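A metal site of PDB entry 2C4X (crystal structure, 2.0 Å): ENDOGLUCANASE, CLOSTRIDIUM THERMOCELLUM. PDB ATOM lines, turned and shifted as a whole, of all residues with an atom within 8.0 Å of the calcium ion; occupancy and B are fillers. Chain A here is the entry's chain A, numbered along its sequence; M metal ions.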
ATOM      1  N   GLY A  98       2.652  29.044  -0.897  1.00  0.00           N
ATOM      2  CA  GLY A  98       2.695  29.975   0.221  1.00  0.00           C
ATOM      3  C   GLY A  98       1.331  30.251   0.850  1.00  0.00           C
ATOM      4  O   GLY A  98       0.314  29.725   0.405  1.00  0.00           O
ATOM      5  N   ASP A  99       1.340  31.097   1.874  1.00  0.00           N
ATOM      6  CA  ASP A  99       0.150  31.386   2.667  1.00  0.00           C
ATOM      7  C   ASP A  99       0.330  32.781   3.248  1.00  0.00           C
ATOM      8  O   ASP A  99       1.159  32.992   4.133  1.00  0.00           O
ATOM      9  CB  ASP A  99       0.021  30.342   3.791  1.00  0.00           C
ATOM     10  CG  ASP A  99      -1.238  30.496   4.619  1.00  0.00           C
ATOM     11  OD1 ASP A  99      -2.001  31.469   4.453  1.00  0.00           O
ATOM     12  OD2 ASP A  99      -1.460  29.614   5.481  1.00  0.00           O
ATOM     13  N   ASN A 100      -0.442  33.729   2.717  1.00  0.00           N
ATOM     14  CA  ASN A 100      -0.382  35.131   3.150  1.00  0.00           C
ATOM     15  C   ASN A 100      -1.434  35.483   4.215  1.00  0.00           C
ATOM     16  O   ASN A 100      -1.727  36.651   4.451  1.00  0.00           O
ATOM     17  CB  ASN A 100      -0.478  36.079   1.942  1.00  0.00           C
ATOM     18  CG  ASN A 100       0.671  35.909   0.970  1.00  0.00           C
ATOM     19  OD1 ASN A 100       0.475  35.883  -0.264  1.00  0.00           O
ATOM     20  ND2 ASN A 100       1.891  35.801   1.501  1.00  0.00           N
ATOM     21  N   SER A 101      -2.001  34.455   4.855  1.00  0.00           N
ATOM     22  CA  SER A 101      -2.985  34.642   5.921  1.00  0.00           C
ATOM     23  C   SER A 101      -2.403  35.436   7.079  1.00  0.00           C
ATOM     24  O   SER A 101      -1.182  35.412   7.309  1.00  0.00           O
ATOM     25  CB  SER A 101      -3.481  33.301   6.451  1.00  0.00           C
ATOM     26  OG  SER A 101      -4.181  32.591   5.450  1.00  0.00           O
ATOM     27  N   PHE A 103      -2.734  34.638  10.135  1.00  0.00           N
ATOM     28  CA  PHE A 103      -2.041  33.553  10.839  1.00  0.00           C
ATOM     29  C   PHE A 103      -1.824  32.384   9.892  1.00  0.00           C
ATOM     30  O   PHE A 103      -2.740  31.596   9.622  1.00  0.00           O
ATOM     31  CB  PHE A 103      -2.774  33.159  12.124  1.00  0.00           C
ATOM     32  CG  PHE A 103      -2.641  34.182  13.215  1.00  0.00           C
ATOM     33  CD1 PHE A 103      -1.503  34.191  14.030  1.00  0.00           C
ATOM     34  CD2 PHE A 103      -3.621  35.144  13.398  1.00  0.00           C
ATOM     35  CE1 PHE A 103      -1.362  35.148  15.044  1.00  0.00           C
ATOM     36  CE2 PHE A 103      -3.488  36.107  14.421  1.00  0.00           C
ATOM     37  CZ  PHE A 103      -2.351  36.110  15.228  1.00  0.00           C
ATOM     38  N   ASN A 104      -0.604  32.311   9.360  1.00  0.00           N
ATOM     39  CA  ASN A 104      -0.270  31.383   8.278  1.00  0.00           C
ATOM     40  C   ASN A 104       0.688  30.281   8.703  1.00  0.00           C
ATOM     41  O   ASN A 104       0.793  29.246   8.030  1.00  0.00           O
ATOM     42  CB  ASN A 104       0.320  32.163   7.089  1.00  0.00           C
ATOM     43  CG  ASN A 104       1.526  33.015   7.475  1.00  0.00           C
ATOM     44  OD1 ASN A 104       2.599  32.485   7.796  1.00  0.00           O
ATOM     45  ND2 ASN A 104       1.359  34.326   7.432  1.00  0.00           N
ATOM     46  N   PHE A 105       1.376  30.522   9.823  1.00  0.00           N
ATOM     47  CA  PHE A 105       2.267  29.569  10.488  1.00  0.00           C
ATOM     48  C   PHE A 105       3.460  29.078   9.659  1.00  0.00           C
ATOM     49  O   PHE A 105       4.105  28.082   9.997  1.00  0.00           O
ATOM     50  CB  PHE A 105       1.450  28.409  11.080  1.00  0.00           C
ATOM     51  CG  PHE A 105       0.322  28.861  11.948  1.00  0.00           C
ATOM     52  CD1 PHE A 105       0.581  29.409  13.211  1.00  0.00           C
ATOM     53  CD2 PHE A 105      -0.999  28.796  11.504  1.00  0.00           C
ATOM     54  CE1 PHE A 105      -0.453  29.862  14.023  1.00  0.00           C
ATOM     55  CE2 PHE A 105      -2.045  29.244  12.311  1.00  0.00           C
ATOM     56  CZ  PHE A 105      -1.777  29.777  13.571  1.00  0.00           C
ATOM     57  N   GLU A 106       3.784  29.821   8.596  1.00  0.00           N
ATOM     58  CA  GLU A 106       4.876  29.444   7.681  1.00  0.00           C
ATOM     59  C   GLU A 106       6.267  29.755   8.233  1.00  0.00           C
ATOM     60  O   GLU A 106       7.275  29.285   7.680  1.00  0.00           O
ATOM     61  CB  GLU A 106       4.682  30.101   6.301  1.00  0.00           C
ATOM     62  CG  GLU A 106       3.326  29.783   5.629  1.00  0.00           C
ATOM     63  CD  GLU A 106       3.140  28.305   5.322  1.00  0.00           C
ATOM     64  OE1 GLU A 106       4.053  27.682   4.756  1.00  0.00           O
ATOM     65  OE2 GLU A 106       2.073  27.757   5.639  1.00  0.00           O
ATOM     66  N   ASP A 107       6.343  30.524   9.313  1.00  0.00           N
ATOM     67  CA  ASP A 107       7.624  30.833   9.951  1.00  0.00           C
ATOM     68  C   ASP A 107       8.048  29.775  10.979  1.00  0.00           C
ATOM     69  O   ASP A 107       9.111  29.884  11.597  1.00  0.00           O
ATOM     70  CB  ASP A 107       7.647  32.245  10.555  1.00  0.00           C
ATOM     71  CG  ASP A 107       6.700  32.401  11.750  1.00  0.00           C
ATOM     72  OD1 ASP A 107       6.021  31.435  12.151  1.00  0.00           O
ATOM     73  OD2 ASP A 107       6.649  33.529  12.294  1.00  0.00           O
ATOM     74  N   ASN A 126       3.752  23.503  15.750  1.00  0.00           N
ATOM     75  CA  ASN A 126       3.781  23.851  14.341  1.00  0.00           C
ATOM     76  C   ASN A 126       4.187  22.627  13.522  1.00  0.00           C
ATOM     77  O   ASN A 126       5.227  22.018  13.756  1.00  0.00           O
ATOM     78  CB  ASN A 126       4.737  25.027  14.103  1.00  0.00           C
ATOM     79  CG  ASN A 126       4.703  25.514  12.662  1.00  0.00           C
ATOM     80  OD1 ASN A 126       5.053  24.772  11.748  1.00  0.00           O
ATOM     81  ND2 ASN A 126       4.302  26.764  12.453  1.00  0.00           N
ATOM     82  N   THR A 127       3.343  22.288  12.538  1.00  0.00           N
ATOM     83  CA  THR A 127       3.449  21.008  11.826  1.00  0.00           C
ATOM     84  C   THR A 127       3.501  21.157  10.307  1.00  0.00           C
ATOM     85  O   THR A 127       2.998  22.136   9.749  1.00  0.00           O
ATOM     86  CB  THR A 127       2.273  20.069  12.195  1.00  0.00           C
ATOM     87  OG1 THR A 127       2.489  18.776  11.626  1.00  0.00           O
ATOM     88  CG2 THR A 127       0.932  20.612  11.689  1.00  0.00           C
ATOM     89  N   LYS A 130      -0.195  18.354   8.134  1.00  0.00           N
ATOM     90  CA  LYS A 130      -1.351  18.876   7.430  1.00  0.00           C
ATOM     91  C   LYS A 130      -1.313  20.398   7.453  1.00  0.00           C
ATOM     92  O   LYS A 130      -0.975  21.009   8.474  1.00  0.00           O
ATOM     93  CB  LYS A 130      -2.664  18.405   8.079  1.00  0.00           C
ATOM     94  CG  LYS A 130      -2.957  16.918   7.957  1.00  0.00           C
ATOM     95  CD  LYS A 130      -4.358  16.586   8.455  1.00  0.00           C
ATOM     96  CE  LYS A 130      -4.490  15.100   8.776  1.00  0.00           C
ATOM     97  NZ  LYS A 130      -4.291  14.218   7.580  1.00  0.00           N
ATOM     98  N   ALA A 131      -1.667  21.014   6.321  1.00  0.00           N
ATOM     99  CA  ALA A 131      -1.835  22.462   6.251  1.00  0.00           C
ATOM    100  C   ALA A 131      -2.975  22.766   5.309  1.00  0.00           C
ATOM    101  O   ALA A 131      -3.270  21.969   4.405  1.00  0.00           O
ATOM    102  CB  ALA A 131      -0.554  23.127   5.785  1.00  0.00           C
ATOM    103  N   PHE A 132      -3.644  23.895   5.527  1.00  0.00           N
ATOM    104  CA  PHE A 132      -4.706  24.337   4.626  1.00  0.00           C
ATOM    105  C   PHE A 132      -4.115  25.102   3.450  1.00  0.00           C
ATOM    106  O   PHE A 132      -4.553  24.934   2.310  1.00  0.00           O
ATOM    107  CB  PHE A 132      -5.775  25.172   5.363  1.00  0.00           C
ATOM    108  CG  PHE A 132      -6.867  25.657   4.455  1.00  0.00           C
ATOM    109  CD1 PHE A 132      -7.875  24.788   4.042  1.00  0.00           C
ATOM    110  CD2 PHE A 132      -6.860  26.965   3.974  1.00  0.00           C
ATOM    111  CE1 PHE A 132      -8.882  25.225   3.176  1.00  0.00           C
ATOM    112  CE2 PHE A 132      -7.857  27.416   3.108  1.00  0.00           C
ATOM    113  CZ  PHE A 132      -8.873  26.547   2.710  1.00  0.00           C
ATOM    114  N   LYS A 133      -3.143  25.958   3.746  1.00  0.00           N
ATOM    115  CA  LYS A 133      -2.400  26.703   2.727  1.00  0.00           C
ATOM    116  C   LYS A 133      -0.935  26.732   3.114  1.00  0.00           C
ATOM    117  O   LYS A 133      -0.604  26.830   4.292  1.00  0.00           O
ATOM    118  CB  LYS A 133      -2.906  28.133   2.616  1.00  0.00           C
ATOM    119  CG  LYS A 133      -3.981  28.343   1.572  1.00  0.00           C
ATOM    120  CD  LYS A 133      -4.106  29.824   1.213  1.00  0.00           C
ATOM    121  CE  LYS A 133      -4.623  30.659   2.377  1.00  0.00           C
ATOM    122  NZ  LYS A 133      -4.910  32.063   1.949  1.00  0.00           N
ATOM    123  N   GLY A 134      -0.060  26.663   2.120  1.00  0.00           N
ATOM    124  CA  GLY A 134       1.366  26.661   2.367  1.00  0.00           C
ATOM    125  C   GLY A 134       1.804  25.305   2.865  1.00  0.00           C
ATOM    126  O   GLY A 134       1.103  24.295   2.651  1.00  0.00           O
ATOM    127  N   GLU A 135       2.943  25.260   3.540  1.00  0.00           N
ATOM    128  CA  GLU A 135       3.496  23.998   3.978  1.00  0.00           C
ATOM    129  C   GLU A 135       3.213  23.687   5.446  1.00  0.00           C
ATOM    130  O   GLU A 135       3.363  22.549   5.875  1.00  0.00           O
ATOM    131  CB  GLU A 135       4.998  23.945   3.668  1.00  0.00           C
ATOM    132  CG  GLU A 135       5.322  23.945   2.173  1.00  0.00           C
ATOM    133  CD  GLU A 135       6.763  24.318   1.887  1.00  0.00           C
ATOM    134  OE1 GLU A 135       7.356  25.079   2.684  1.00  0.00           O
ATOM    135  OE2 GLU A 135       7.313  23.863   0.852  1.00  0.00           O
ATOM    136  N   ARG A 136       2.766  24.682   6.204  1.00  0.00           N
ATOM    137  CA  ARG A 136       2.676  24.552   7.658  1.00  0.00           C
ATOM    138  C   ARG A 136       1.351  25.006   8.259  1.00  0.00           C
ATOM    139  O   ARG A 136       0.615  25.767   7.645  1.00  0.00           O
ATOM    140  CB  ARG A 136       3.837  25.286   8.328  1.00  0.00           C
ATOM    141  CG  ARG A 136       5.199  24.720   8.021  1.00  0.00           C
ATOM    142  CD  ARG A 136       6.303  25.490   8.708  1.00  0.00           C
ATOM    143  NE  ARG A 136       7.560  24.777   8.613  1.00  0.00           N
ATOM    144  CZ  ARG A 136       7.996  23.871   9.493  1.00  0.00           C
ATOM    145  NH1 ARG A 136       7.268  23.576  10.570  1.00  0.00           N
ATOM    146  NH2 ARG A 136       9.160  23.267   9.289  1.00  0.00           N
ATOM    147  N   GLY A 137       1.072  24.528   9.471  1.00  0.00           N
ATOM    148  CA  GLY A 137      -0.089  24.951  10.248  1.00  0.00           C
ATOM    149  C   GLY A 137       0.137  24.531  11.683  1.00  0.00           C
ATOM    150  O   GLY A 137       1.262  24.201  12.062  1.00  0.00           O
ATOM    151  N   LEU A 138      -0.926  24.547  12.484  1.00  0.00           N
ATOM    152  CA  LEU A 138      -0.849  24.069  13.870  1.00  0.00           C
ATOM    153  C   LEU A 138      -1.422  22.665  13.983  1.00  0.00           C
ATOM    154  O   LEU A 138      -2.361  22.297  13.267  1.00  0.00           O
ATOM    155  CB  LEU A 138      -1.572  25.008  14.840  1.00  0.00           C
ATOM    156  CG  LEU A 138      -0.989  26.412  15.032  1.00  0.00           C
ATOM    157  CD1 LEU A 138      -1.750  27.181  16.117  1.00  0.00           C
ATOM    158  CD2 LEU A 138       0.518  26.360  15.365  1.00  0.00           C
ATOM    159  N   TRP A 212     -11.079  19.653   6.123  1.00  0.00           N
ATOM    160  CA  TRP A 212     -10.967  21.058   6.493  1.00  0.00           C
ATOM    161  C   TRP A 212     -12.331  21.712   6.548  1.00  0.00           C
ATOM    162  O   TRP A 212     -13.143  21.574   5.624  1.00  0.00           O
ATOM    163  CB  TRP A 212     -10.046  21.802   5.515  1.00  0.00           C
ATOM    164  CG  TRP A 212      -8.595  21.477   5.693  1.00  0.00           C
ATOM    165  CD1 TRP A 212      -7.826  20.668   4.898  1.00  0.00           C
ATOM    166  CD2 TRP A 212      -7.730  21.945   6.748  1.00  0.00           C
ATOM    167  NE1 TRP A 212      -6.531  20.610   5.386  1.00  0.00           N
ATOM    168  CE2 TRP A 212      -6.448  21.383   6.517  1.00  0.00           C
ATOM    169  CE3 TRP A 212      -7.922  22.784   7.847  1.00  0.00           C
ATOM    170  CZ2 TRP A 212      -5.364  21.640   7.349  1.00  0.00           C
ATOM    171  CZ3 TRP A 212      -6.838  23.042   8.680  1.00  0.00           C
ATOM    172  CH2 TRP A 212      -5.579  22.460   8.429  1.00  0.00           C
ATOM    173  N   VAL A 247      -5.185  23.368  12.623  1.00  0.00           N
ATOM    174  CA  VAL A 247      -5.646  24.750  12.481  1.00  0.00           C
ATOM    175  C   VAL A 247      -4.649  25.512  11.623  1.00  0.00           C
ATOM    176  O   VAL A 247      -3.439  25.446  11.850  1.00  0.00           O
ATOM    177  CB  VAL A 247      -5.765  25.477  13.842  1.00  0.00           C
ATOM    178  CG1 VAL A 247      -6.272  26.906  13.652  1.00  0.00           C
ATOM    179  CG2 VAL A 247      -6.687  24.698  14.811  1.00  0.00           C
ATOM    180  N   ASP A 248      -5.154  26.244  10.625  1.00  0.00           N
ATOM    181  CA  ASP A 248      -4.275  26.977   9.716  1.00  0.00           C
ATOM    182  C   ASP A 248      -5.023  28.083   9.042  1.00  0.00           C
ATOM    183  O   ASP A 248      -6.253  28.054   8.982  1.00  0.00           O
ATOM    184  CB  ASP A 248      -3.677  26.042   8.642  1.00  0.00           C
ATOM    185  CG  ASP A 248      -2.528  26.688   7.877  1.00  0.00           C
ATOM    186  OD1 ASP A 248      -1.906  27.636   8.411  1.00  0.00           O
ATOM    187  OD2 ASP A 248      -2.212  26.245   6.746  1.00  0.00           O
ATOM    188  N   ALA A 249      -4.267  29.069   8.546  1.00  0.00           N
ATOM    189  CA  ALA A 249      -4.775  30.092   7.642  1.00  0.00           C
ATOM    190  C   ALA A 249      -5.946  30.876   8.224  1.00  0.00           C
ATOM    191  O   ALA A 249      -6.961  31.103   7.545  1.00  0.00           O
ATOM    192  CB  ALA A 249      -5.120  29.483   6.272  1.00  0.00           C
ATOM    193  N   ILE A 250      -5.811  31.277   9.485  1.00  0.00           N
ATOM    194  CA  ILE A 250      -6.753  32.217  10.098  1.00  0.00           C
ATOM    195  C   ILE A 250      -6.514  33.586   9.462  1.00  0.00           C
ATOM    196  O   ILE A 250      -5.381  34.078   9.424  1.00  0.00           O
ATOM    197  CB  ILE A 250      -6.607  32.296  11.629  1.00  0.00           C
ATOM    198  CG1 ILE A 250      -6.719  30.896  12.246  1.00  0.00           C
ATOM    199  CG2 ILE A 250      -7.674  33.218  12.221  1.00  0.00           C
ATOM    200  CD1 ILE A 250      -6.291  30.830  13.715  1.00  0.00           C
HETATM  201 CA    CA M   1      -0.196  27.715   6.481  1.00  0.00          CA
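N of Glu 135 is in hydrogen-bond range of OE1 of Glu 106 (2.9 Å). OD2 of Asp 248 lies close to N of Phe 132 (3.0 Å). The backbone carbonyl oxygen (O) of Ser 101 is in hydrogen-bond range of the side-chain amide nitrogen (ND2) of Asn 104 (2.8 Å). The guanidinium group (NH1) of Arg 136 sits at hydrogen-bond distance from the side-chain amide oxygen (OD1) of Asn 126 (2.8 Å). The side-chain carboxylate of Asp 99 sits at hydrogen-bond distance from the side-chain hydroxyl of Ser 101 (2.6 Å).
Six residues have an atom within 4 Å of the calcium ion: Asp 99, Asn 104, Glu 106, Lys 133, Arg 136 and Asp 248. The nearest printed residue that does not touch the calcium ion is Gly 134 (4.5 Å).
The calcium ion is bound by the backbone carbonyl oxygen (O) of Asn 104 (2.4 Å), the backbone carbonyl oxygen (O) of Lys 133 (2.4 Å), the backbone carbonyl oxygen (O) of Arg 136 (2.4 Å), the side-chain carboxylate (OE2) of Glu 106 (2.4 Å), the side-chain carboxylate (OD2) of Asp 99 (2.5 Å), the side-chain carboxylate (OD2) of Asp 248 (2.5 Å) and the side-chain carboxylate (OD1) of Asp 248 (2.6 Å). The calcium ion has seven donor atoms within binding distance.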
